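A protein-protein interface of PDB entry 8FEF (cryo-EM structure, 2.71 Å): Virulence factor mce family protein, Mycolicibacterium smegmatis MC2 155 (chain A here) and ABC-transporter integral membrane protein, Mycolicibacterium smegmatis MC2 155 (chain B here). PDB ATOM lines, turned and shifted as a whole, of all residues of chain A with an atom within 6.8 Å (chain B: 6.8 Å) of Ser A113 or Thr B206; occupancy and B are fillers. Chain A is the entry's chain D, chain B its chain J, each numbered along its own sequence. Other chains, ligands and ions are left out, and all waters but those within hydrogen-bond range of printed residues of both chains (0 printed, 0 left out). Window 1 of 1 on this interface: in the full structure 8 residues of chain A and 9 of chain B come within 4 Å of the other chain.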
ATOM      1  N   ALA A  58     -14.426   9.419  -5.887  1.00  0.00           N
ATOM      2  CA  ALA A  58     -15.802   9.677  -5.467  1.00  0.00           C
ATOM      3  C   ALA A  58     -16.540  10.609  -6.421  1.00  0.00           C
ATOM      4  O   ALA A  58     -17.515  11.259  -6.033  1.00  0.00           O
ATOM      5  CB  ALA A  58     -15.860  10.229  -4.038  1.00  0.00           C
ATOM      6  N   LEU A  59     -16.086  10.684  -7.666  1.00  0.00           N
ATOM      7  CA  LEU A  59     -16.743  11.448  -8.715  1.00  0.00           C
ATOM      8  C   LEU A  59     -17.269  10.468  -9.751  1.00  0.00           C
ATOM      9  O   LEU A  59     -16.514   9.632 -10.257  1.00  0.00           O
ATOM     10  CB  LEU A  59     -15.778  12.446  -9.354  1.00  0.00           C
ATOM     11  CG  LEU A  59     -16.375  13.521 -10.256  1.00  0.00           C
ATOM     12  CD1 LEU A  59     -17.062  14.578  -9.416  1.00  0.00           C
ATOM     13  CD2 LEU A  59     -15.306  14.137 -11.136  1.00  0.00           C
ATOM     14  N   TYR A  60     -18.554  10.562 -10.053  1.00  0.00           N
ATOM     15  CA  TYR A  60     -19.239   9.611 -10.912  1.00  0.00           C
ATOM     16  C   TYR A  60     -19.965  10.353 -12.019  1.00  0.00           C
ATOM     17  O   TYR A  60     -20.274  11.541 -11.880  1.00  0.00           O
ATOM     18  CB  TYR A  60     -20.240   8.774 -10.100  1.00  0.00           C
ATOM     19  CG  TYR A  60     -19.736   8.395  -8.729  1.00  0.00           C
ATOM     20  CD1 TYR A  60     -18.803   7.382  -8.567  1.00  0.00           C
ATOM     21  CD2 TYR A  60     -20.196   9.048  -7.598  1.00  0.00           C
ATOM     22  CE1 TYR A  60     -18.339   7.036  -7.317  1.00  0.00           C
ATOM     23  CE2 TYR A  60     -19.741   8.707  -6.343  1.00  0.00           C
ATOM     24  CZ  TYR A  60     -18.812   7.701  -6.208  1.00  0.00           C
ATOM     25  OH  TYR A  60     -18.355   7.359  -4.957  1.00  0.00           O
ATOM     26  N   PRO A  61     -20.219   9.692 -13.150  1.00  0.00           N
ATOM     27  CA  PRO A  61     -21.032  10.316 -14.199  1.00  0.00           C
ATOM     28  C   PRO A  61     -22.410  10.689 -13.675  1.00  0.00           C
ATOM     29  O   PRO A  61     -23.035   9.937 -12.925  1.00  0.00           O
ATOM     30  CB  PRO A  61     -21.110   9.232 -15.278  1.00  0.00           C
ATOM     31  CG  PRO A  61     -19.886   8.420 -15.071  1.00  0.00           C
ATOM     32  CD  PRO A  61     -19.655   8.403 -13.589  1.00  0.00           C
ATOM     33  N   GLY A  62     -22.883  11.860 -14.085  1.00  0.00           N
ATOM     34  CA  GLY A  62     -24.118  12.403 -13.571  1.00  0.00           C
ATOM     35  C   GLY A  62     -23.959  13.362 -12.412  1.00  0.00           C
ATOM     36  O   GLY A  62     -24.944  13.997 -12.019  1.00  0.00           O
ATOM     37  N   ASP A  63     -22.758  13.488 -11.852  1.00  0.00           N
ATOM     38  CA  ASP A  63     -22.522  14.464 -10.800  1.00  0.00           C
ATOM     39  C   ASP A  63     -22.584  15.878 -11.366  1.00  0.00           C
ATOM     40  O   ASP A  63     -22.352  16.107 -12.554  1.00  0.00           O
ATOM     41  CB  ASP A  63     -21.173  14.222 -10.126  1.00  0.00           C
ATOM     42  CG  ASP A  63     -21.253  13.190  -9.017  1.00  0.00           C
ATOM     43  OD1 ASP A  63     -22.353  12.648  -8.787  1.00  0.00           O
ATOM     44  OD2 ASP A  63     -20.221  12.924  -8.369  1.00  0.00           O
ATOM     45  N   LYS A  64     -22.901  16.830 -10.494  1.00  0.00           N
ATOM     46  CA  LYS A  64     -23.217  18.181 -10.928  1.00  0.00           C
ATOM     47  C   LYS A  64     -21.959  18.976 -11.254  1.00  0.00           C
ATOM     48  O   LYS A  64     -20.886  18.751 -10.689  1.00  0.00           O
ATOM     49  CB  LYS A  64     -24.021  18.910  -9.852  1.00  0.00           C
ATOM     50  CG  LYS A  64     -25.245  18.148  -9.376  1.00  0.00           C
ATOM     51  CD  LYS A  64     -26.149  17.774 -10.536  1.00  0.00           C
ATOM     52  CE  LYS A  64     -27.310  16.915 -10.074  1.00  0.00           C
ATOM     53  NZ  LYS A  64     -28.191  16.528 -11.209  1.00  0.00           N
ATOM     54  N   ARG A  71     -25.709  25.055 -10.005  1.00  0.00           N
ATOM     55  CA  ARG A  71     -25.665  23.988 -10.999  1.00  0.00           C
ATOM     56  C   ARG A  71     -25.854  24.550 -12.401  1.00  0.00           C
ATOM     57  O   ARG A  71     -26.778  25.329 -12.652  1.00  0.00           O
ATOM     58  CB  ARG A  71     -26.744  22.947 -10.707  1.00  0.00           C
ATOM     59  CG  ARG A  71     -26.617  22.260  -9.362  1.00  0.00           C
ATOM     60  CD  ARG A  71     -27.707  21.214  -9.190  1.00  0.00           C
ATOM     61  NE  ARG A  71     -27.573  20.474  -7.940  1.00  0.00           N
ATOM     62  CZ  ARG A  71     -28.359  19.467  -7.581  1.00  0.00           C
ATOM     63  NH1 ARG A  71     -29.350  19.054  -8.354  1.00  0.00           N
ATOM     64  NH2 ARG A  71     -28.144  18.859  -6.418  1.00  0.00           N
ATOM     65  N   LEU A 106     -14.571  19.521  -6.177  1.00  0.00           N
ATOM     66  CA  LEU A 106     -14.873  19.962  -4.825  1.00  0.00           C
ATOM     67  C   LEU A 106     -15.653  18.890  -4.082  1.00  0.00           C
ATOM     68  O   LEU A 106     -16.547  18.250  -4.646  1.00  0.00           O
ATOM     69  CB  LEU A 106     -15.677  21.266  -4.832  1.00  0.00           C
ATOM     70  CG  LEU A 106     -15.034  22.490  -5.480  1.00  0.00           C
ATOM     71  CD1 LEU A 106     -16.007  23.650  -5.480  1.00  0.00           C
ATOM     72  CD2 LEU A 106     -13.756  22.867  -4.757  1.00  0.00           C
ATOM     73  N   ASN A 107     -15.303  18.708  -2.809  1.00  0.00           N
ATOM     74  CA  ASN A 107     -16.059  17.876  -1.882  1.00  0.00           C
ATOM     75  C   ASN A 107     -16.785  18.805  -0.919  1.00  0.00           C
ATOM     76  O   ASN A 107     -16.172  19.313   0.032  1.00  0.00           O
ATOM     77  CB  ASN A 107     -15.134  16.922  -1.122  1.00  0.00           C
ATOM     78  CG  ASN A 107     -15.895  15.889  -0.319  1.00  0.00           C
ATOM     79  OD1 ASN A 107     -17.081  15.661  -0.545  1.00  0.00           O
ATOM     80  ND2 ASN A 107     -15.212  15.256   0.626  1.00  0.00           N
ATOM     81  N   PRO A 108     -18.079  19.074  -1.133  1.00  0.00           N
ATOM     82  CA  PRO A 108     -18.744  20.155  -0.382  1.00  0.00           C
ATOM     83  C   PRO A 108     -18.767  19.968   1.127  1.00  0.00           C
ATOM     84  O   PRO A 108     -18.672  20.958   1.861  1.00  0.00           O
ATOM     85  CB  PRO A 108     -20.161  20.155  -0.972  1.00  0.00           C
ATOM     86  CG  PRO A 108     -20.006  19.554  -2.326  1.00  0.00           C
ATOM     87  CD  PRO A 108     -18.950  18.508  -2.174  1.00  0.00           C
ATOM     88  N   SER A 109     -18.893  18.739   1.618  1.00  0.00           N
ATOM     89  CA  SER A 109     -19.010  18.517   3.053  1.00  0.00           C
ATOM     90  C   SER A 109     -18.424  17.151   3.388  1.00  0.00           C
ATOM     91  O   SER A 109     -17.738  16.534   2.568  1.00  0.00           O
ATOM     92  CB  SER A 109     -20.468  18.650   3.508  1.00  0.00           C
ATOM     93  OG  SER A 109     -21.302  17.718   2.845  1.00  0.00           O
ATOM     94  N   VAL A 111     -20.008  14.201   4.033  1.00  0.00           N
ATOM     95  CA  VAL A 111     -20.652  13.241   3.147  1.00  0.00           C
ATOM     96  C   VAL A 111     -21.464  14.042   2.143  1.00  0.00           C
ATOM     97  O   VAL A 111     -22.487  14.641   2.497  1.00  0.00           O
ATOM     98  CB  VAL A 111     -21.540  12.252   3.910  1.00  0.00           C
ATOM     99  CG1 VAL A 111     -22.296  11.365   2.937  1.00  0.00           C
ATOM    100  CG2 VAL A 111     -20.705  11.419   4.866  1.00  0.00           C
ATOM    101  N   ALA A 112     -21.014  14.056   0.894  1.00  0.00           N
ATOM    102  CA  ALA A 112     -21.679  14.823  -0.149  1.00  0.00           C
ATOM    103  C   ALA A 112     -21.354  14.187  -1.492  1.00  0.00           C
ATOM    104  O   ALA A 112     -20.601  13.215  -1.577  1.00  0.00           O
ATOM    105  CB  ALA A 112     -21.257  16.294  -0.110  1.00  0.00           C
ATOM    106  N   SER A 113     -21.939  14.745  -2.545  1.00  0.00           N
ATOM    107  CA  SER A 113     -21.628  14.356  -3.911  1.00  0.00           C
ATOM    108  C   SER A 113     -20.632  15.361  -4.471  1.00  0.00           C
ATOM    109  O   SER A 113     -20.931  16.556  -4.551  1.00  0.00           O
ATOM    110  CB  SER A 113     -22.891  14.305  -4.769  1.00  0.00           C
ATOM    111  OG  SER A 113     -23.499  15.579  -4.864  1.00  0.00           O
ATOM    112  N   ARG A 114     -19.448  14.878  -4.837  1.00  0.00           N
ATOM    113  CA  ARG A 114     -18.399  15.761  -5.320  1.00  0.00           C
ATOM    114  C   ARG A 114     -18.796  16.381  -6.652  1.00  0.00           C
ATOM    115  O   ARG A 114     -19.457  15.749  -7.478  1.00  0.00           O
ATOM    116  CB  ARG A 114     -17.086  14.997  -5.457  1.00  0.00           C
ATOM    117  CG  ARG A 114     -16.690  14.277  -4.189  1.00  0.00           C
ATOM    118  CD  ARG A 114     -15.225  13.915  -4.193  1.00  0.00           C
ATOM    119  NE  ARG A 114     -14.827  13.310  -2.929  1.00  0.00           N
ATOM    120  CZ  ARG A 114     -13.580  13.000  -2.609  1.00  0.00           C
ATOM    121  NH1 ARG A 114     -12.578  13.229  -3.441  1.00  0.00           N
ATOM    122  NH2 ARG A 114     -13.331  12.448  -1.426  1.00  0.00           N
ATOM    123  N   VAL A 115     -18.396  17.633  -6.851  1.00  0.00           N
ATOM    124  CA  VAL A 115     -18.802  18.405  -8.015  1.00  0.00           C
ATOM    125  C   VAL A 115     -17.557  18.903  -8.734  1.00  0.00           C
ATOM    126  O   VAL A 115     -16.443  18.811  -8.228  1.00  0.00           O
ATOM    127  CB  VAL A 115     -19.716  19.584  -7.636  1.00  0.00           C
ATOM    128  CG1 VAL A 115     -20.973  19.084  -6.946  1.00  0.00           C
ATOM    129  CG2 VAL A 115     -18.967  20.550  -6.740  1.00  0.00           C
ATOM    130  N   GLU B 106     -26.840  13.306   3.263  1.00  0.00           N
ATOM    131  CA  GLU B 106     -27.916  12.933   2.353  1.00  0.00           C
ATOM    132  C   GLU B 106     -27.439  12.146   1.141  1.00  0.00           C
ATOM    133  O   GLU B 106     -28.269  11.722   0.332  1.00  0.00           O
ATOM    134  CB  GLU B 106     -28.670  14.182   1.890  1.00  0.00           C
ATOM    135  CG  GLU B 106     -27.780  15.241   1.271  1.00  0.00           C
ATOM    136  CD  GLU B 106     -28.484  16.569   1.106  1.00  0.00           C
ATOM    137  OE1 GLU B 106     -29.720  16.611   1.271  1.00  0.00           O
ATOM    138  OE2 GLU B 106     -27.801  17.573   0.816  1.00  0.00           O
ATOM    139  N   ALA B 107     -26.132  11.943   0.989  1.00  0.00           N
ATOM    140  CA  ALA B 107     -25.619  11.116  -0.096  1.00  0.00           C
ATOM    141  C   ALA B 107     -25.788   9.629   0.172  1.00  0.00           C
ATOM    142  O   ALA B 107     -25.589   8.823  -0.743  1.00  0.00           O
ATOM    143  CB  ALA B 107     -24.144  11.430  -0.347  1.00  0.00           C
ATOM    144  N   PHE B 108     -26.156   9.251   1.393  1.00  0.00           N
ATOM    145  CA  PHE B 108     -26.352   7.861   1.776  1.00  0.00           C
ATOM    146  C   PHE B 108     -27.745   7.342   1.446  1.00  0.00           C
ATOM    147  O   PHE B 108     -28.050   6.192   1.783  1.00  0.00           O
ATOM    148  CB  PHE B 108     -26.090   7.684   3.274  1.00  0.00           C
ATOM    149  CG  PHE B 108     -24.647   7.825   3.662  1.00  0.00           C
ATOM    150  CD1 PHE B 108     -23.640   7.643   2.732  1.00  0.00           C
ATOM    151  CD2 PHE B 108     -24.298   8.128   4.967  1.00  0.00           C
ATOM    152  CE1 PHE B 108     -22.314   7.766   3.094  1.00  0.00           C
ATOM    153  CE2 PHE B 108     -22.974   8.254   5.333  1.00  0.00           C
ATOM    154  CZ  PHE B 108     -21.982   8.072   4.394  1.00  0.00           C
ATOM    155  N   GLY B 110     -29.227   6.380  -1.329  1.00  0.00           N
ATOM    156  CA  GLY B 110     -29.182   5.150  -2.107  1.00  0.00           C
ATOM    157  C   GLY B 110     -28.764   3.956  -1.274  1.00  0.00           C
ATOM    158  O   GLY B 110     -29.249   2.842  -1.478  1.00  0.00           O
ATOM    159  N   PHE B 111     -27.854   4.174  -0.326  1.00  0.00           N
ATOM    160  CA  PHE B 111     -27.496   3.114   0.607  1.00  0.00           C
ATOM    161  C   PHE B 111     -28.637   2.830   1.576  1.00  0.00           C
ATOM    162  O   PHE B 111     -28.876   1.673   1.939  1.00  0.00           O
ATOM    163  CB  PHE B 111     -26.216   3.499   1.354  1.00  0.00           C
ATOM    164  CG  PHE B 111     -26.240   3.174   2.821  1.00  0.00           C
ATOM    165  CD1 PHE B 111     -26.019   1.883   3.268  1.00  0.00           C
ATOM    166  CD2 PHE B 111     -26.475   4.169   3.754  1.00  0.00           C
ATOM    167  CE1 PHE B 111     -26.050   1.595   4.614  1.00  0.00           C
ATOM    168  CE2 PHE B 111     -26.502   3.882   5.102  1.00  0.00           C
ATOM    169  CZ  PHE B 111     -26.287   2.595   5.533  1.00  0.00           C
ATOM    170  N   GLN B 202     -31.131  14.719  -6.724  1.00  0.00           N
ATOM    171  CA  GLN B 202     -29.833  14.141  -6.413  1.00  0.00           C
ATOM    172  C   GLN B 202     -29.206  13.568  -7.680  1.00  0.00           C
ATOM    173  O   GLN B 202     -29.902  13.086  -8.577  1.00  0.00           O
ATOM    174  CB  GLN B 202     -29.967  13.054  -5.343  1.00  0.00           C
ATOM    175  CG  GLN B 202     -28.638  12.464  -4.887  1.00  0.00           C
ATOM    176  CD  GLN B 202     -28.780  11.493  -3.736  1.00  0.00           C
ATOM    177  OE1 GLN B 202     -29.055  10.312  -3.936  1.00  0.00           O
ATOM    178  NE2 GLN B 202     -28.587  11.986  -2.520  1.00  0.00           N
ATOM    179  N   SER B 203     -27.879  13.644  -7.758  1.00  0.00           N
ATOM    180  CA  SER B 203     -27.171  13.119  -8.917  1.00  0.00           C
ATOM    181  C   SER B 203     -27.352  11.611  -9.011  1.00  0.00           C
ATOM    182  O   SER B 203     -27.367  10.905  -7.999  1.00  0.00           O
ATOM    183  CB  SER B 203     -25.686  13.468  -8.836  1.00  0.00           C
ATOM    184  OG  SER B 203     -25.085  12.859  -7.709  1.00  0.00           O
ATOM    185  N   VAL B 204     -27.502  11.117 -10.242  1.00  0.00           N
ATOM    186  CA  VAL B 204     -27.731   9.690 -10.440  1.00  0.00           C
ATOM    187  C   VAL B 204     -26.465   8.889 -10.149  1.00  0.00           C
ATOM    188  O   VAL B 204     -26.543   7.736  -9.709  1.00  0.00           O
ATOM    189  CB  VAL B 204     -28.273   9.433 -11.861  1.00  0.00           C
ATOM    190  CG1 VAL B 204     -27.245   9.801 -12.920  1.00  0.00           C
ATOM    191  CG2 VAL B 204     -28.727   7.989 -12.015  1.00  0.00           C
ATOM    192  N   GLY B 205     -25.289   9.479 -10.375  1.00  0.00           N
ATOM    193  CA  GLY B 205     -24.049   8.755 -10.136  1.00  0.00           C
ATOM    194  C   GLY B 205     -23.846   8.403  -8.676  1.00  0.00           C
ATOM    195  O   GLY B 205     -23.490   7.271  -8.341  1.00  0.00           O
ATOM    196  N   THR B 206     -24.067   9.374  -7.787  1.00  0.00           N
ATOM    197  CA  THR B 206     -23.919   9.127  -6.356  1.00  0.00           C
ATOM    198  C   THR B 206     -24.927   8.096  -5.865  1.00  0.00           C
ATOM    199  O   THR B 206     -24.580   7.196  -5.086  1.00  0.00           O
ATOM    200  CB  THR B 206     -24.073  10.440  -5.589  1.00  0.00           C
ATOM    201  OG1 THR B 206     -23.071  11.362  -6.026  1.00  0.00           O
ATOM    202  CG2 THR B 206     -23.928  10.215  -4.095  1.00  0.00           C
ATOM    203  N   TYR B 207     -26.180   8.211  -6.312  1.00  0.00           N
ATOM    204  CA  TYR B 207     -27.203   7.253  -5.908  1.00  0.00           C
ATOM    205  C   TYR B 207     -26.845   5.849  -6.374  1.00  0.00           C
ATOM    206  O   TYR B 207     -26.931   4.889  -5.604  1.00  0.00           O
ATOM    207  CB  TYR B 207     -28.571   7.671  -6.454  1.00  0.00           C
ATOM    208  CG  TYR B 207     -29.715   6.818  -5.940  1.00  0.00           C
ATOM    209  CD1 TYR B 207     -30.039   5.607  -6.541  1.00  0.00           C
ATOM    210  CD2 TYR B 207     -30.459   7.218  -4.841  1.00  0.00           C
ATOM    211  CE1 TYR B 207     -31.066   4.829  -6.064  1.00  0.00           C
ATOM    212  CE2 TYR B 207     -31.495   6.446  -4.362  1.00  0.00           C
ATOM    213  CZ  TYR B 207     -31.791   5.254  -4.975  1.00  0.00           C
ATOM    214  OH  TYR B 207     -32.821   4.480  -4.498  1.00  0.00           O
ATOM    215  N   GLU B 208     -26.443   5.713  -7.641  1.00  0.00           N
ATOM    216  CA  GLU B 208     -26.105   4.397  -8.171  1.00  0.00           C
ATOM    217  C   GLU B 208     -24.881   3.817  -7.478  1.00  0.00           C
ATOM    218  O   GLU B 208     -24.828   2.609  -7.222  1.00  0.00           O
ATOM    219  CB  GLU B 208     -25.891   4.472  -9.679  1.00  0.00           C
ATOM    220  CG  GLU B 208     -27.175   4.638 -10.471  1.00  0.00           C
ATOM    221  CD  GLU B 208     -26.947   4.596 -11.965  1.00  0.00           C
ATOM    222  OE1 GLU B 208     -25.774   4.514 -12.386  1.00  0.00           O
ATOM    223  OE2 GLU B 208     -27.940   4.646 -12.720  1.00  0.00           O
ATOM    224  N   HIS B 209     -23.891   4.656  -7.161  1.00  0.00           N
ATOM    225  CA  HIS B 209     -22.718   4.169  -6.443  1.00  0.00           C
ATOM    226  C   HIS B 209     -23.100   3.640  -5.068  1.00  0.00           C
ATOM    227  O   HIS B 209     -22.754   2.508  -4.709  1.00  0.00           O
ATOM    228  CB  HIS B 209     -21.676   5.276  -6.313  1.00  0.00           C
ATOM    229  CG  HIS B 209     -20.515   4.902  -5.446  1.00  0.00           C
ATOM    230  ND1 HIS B 209     -19.432   4.193  -5.920  1.00  0.00           N
ATOM    231  CD2 HIS B 209     -20.276   5.120  -4.132  1.00  0.00           C
ATOM    232  CE1 HIS B 209     -18.570   4.002  -4.937  1.00  0.00           C
ATOM    233  NE2 HIS B 209     -19.059   4.554  -3.842  1.00  0.00           N
ATOM    234  N   TYR B 210     -23.821   4.443  -4.283  1.00  0.00           N
ATOM    235  CA  TYR B 210     -24.158   4.011  -2.933  1.00  0.00           C
ATOM    236  C   TYR B 210     -25.202   2.904  -2.928  1.00  0.00           C
ATOM    237  O   TYR B 210     -25.362   2.226  -1.908  1.00  0.00           O
ATOM    238  CB  TYR B 210     -24.631   5.198  -2.098  1.00  0.00           C
ATOM    239  CG  TYR B 210     -23.493   6.058  -1.606  1.00  0.00           C
ATOM    240  CD1 TYR B 210     -22.738   5.676  -0.509  1.00  0.00           C
ATOM    241  CD2 TYR B 210     -23.164   7.242  -2.246  1.00  0.00           C
ATOM    242  CE1 TYR B 210     -21.693   6.451  -0.060  1.00  0.00           C
ATOM    243  CE2 TYR B 210     -22.120   8.026  -1.803  1.00  0.00           C
ATOM    244  CZ  TYR B 210     -21.388   7.626  -0.710  1.00  0.00           C
ATOM    245  OH  TYR B 210     -20.346   8.403  -0.263  1.00  0.00           O
ATOM    246  N   PHE B 211     -25.910   2.706  -4.040  1.00  0.00           N
ATOM    247  CA  PHE B 211     -26.862   1.610  -4.143  1.00  0.00           C
ATOM    248  C   PHE B 211     -26.157   0.303  -4.487  1.00  0.00           C
ATOM    249  O   PHE B 211     -26.337  -0.706  -3.801  1.00  0.00           O
ATOM    250  CB  PHE B 211     -27.927   1.951  -5.188  1.00  0.00           C
ATOM    251  CG  PHE B 211     -28.873   0.826  -5.490  1.00  0.00           C
ATOM    252  CD1 PHE B 211     -29.883   0.498  -4.606  1.00  0.00           C
ATOM    253  CD2 PHE B 211     -28.761   0.109  -6.666  1.00  0.00           C
ATOM    254  CE1 PHE B 211     -30.753  -0.533  -4.886  1.00  0.00           C
ATOM    255  CE2 PHE B 211     -29.629  -0.923  -6.948  1.00  0.00           C
ATOM    256  CZ  PHE B 211     -30.625  -1.244  -6.057  1.00  0.00           C
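The side-chain hydroxyl of Tyr A60 sits close to a ring nitrogen (NE2) of His B209, at 3.1 Å.
The backbone carbonyl oxygen (O) of Pro A61 sits close to the backbone NH (N) of Gly B205 (3.4 Å).
OD1 of Asp A63 sits at hydrogen-bond distance from OG of Ser B203, 2.9 Å away.
The side-chain carboxylate (OD1) of Asp A63 lies within hydrogen-bond range of the side-chain hydroxyl (OG1) of Thr B206, 3.1 Å away.
The backbone NH (N) of Tyr A60 sits at hydrogen-bond distance from the side-chain carboxylate (OD2) of Asp A63 (3.3 Å).
The side-chain hydroxyl (OG) of Ser A109 sits at hydrogen-bond distance from the backbone carbonyl oxygen (O) of Val A111 (3.3 Å).
The side-chain hydroxyl (OG1) of Thr B206 lies within hydrogen-bond range of the side-chain hydroxyl (OG) of Ser B203, 3.0 Å away.
Among the printed residues, pairs that only touch across the chains: Ser A113 with Thr B206 (3.2 Å), Gly A62 with Ser B203 (3.3 Å), Val A111 with Phe B108 (3.6 Å), Val A111 with Ala B107 (3.8 Å), Tyr A60 with Gly B205 (3.8 Å), Tyr A60 with Thr B206 (3.9 Å), Ser A113 with Ser B203 (3.9 Å) and Lys A64 with Ser B203 (3.97 Å).
Ser A113 touches two residues of chain B.
Of chain A, only Tyr A60, Asp A63 and Ser A113 come within 4 Å of Thr B206.
Of the printed residues of chain B, Lys A64 touches Ser B203.
Of the printed residues of chain A, Ala B107 touches Val A111.
The nearest residue of chain B that does not touch Ser A113 is Ala B107 (4.5 Å).
The nearest printed residue of chain B that does not touch Lys A64 is Gln B202 (4.5 Å).
Of the 15 printed residues of chain B, 6 touch a printed residue of chain A.
Printed residues of chain B that touch a printed residue of chain A: Ala B107, Phe B108, Ser B203, Gly B205, Thr B206 and His B209.
Hydrophobic or aromatic side chains of chain B within 4 Å of the printed part of chain A: Ala B107, Phe B108 and His B209.
Of the 17 printed residues of chain A, 7 touch a printed residue of chain B.
Printed residues of chain A that touch a printed residue of chain B: Tyr A60, Pro A61, Gly A62, Asp A63, Lys A64, Val A111 and Ser A113.
Among the printed residues, 12 pairs touch across the chains.
Among the printed residues, no Asp or Glu carboxylate lies within 4 Å of a Lys or Arg side-chain nitrogen of the other chain.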
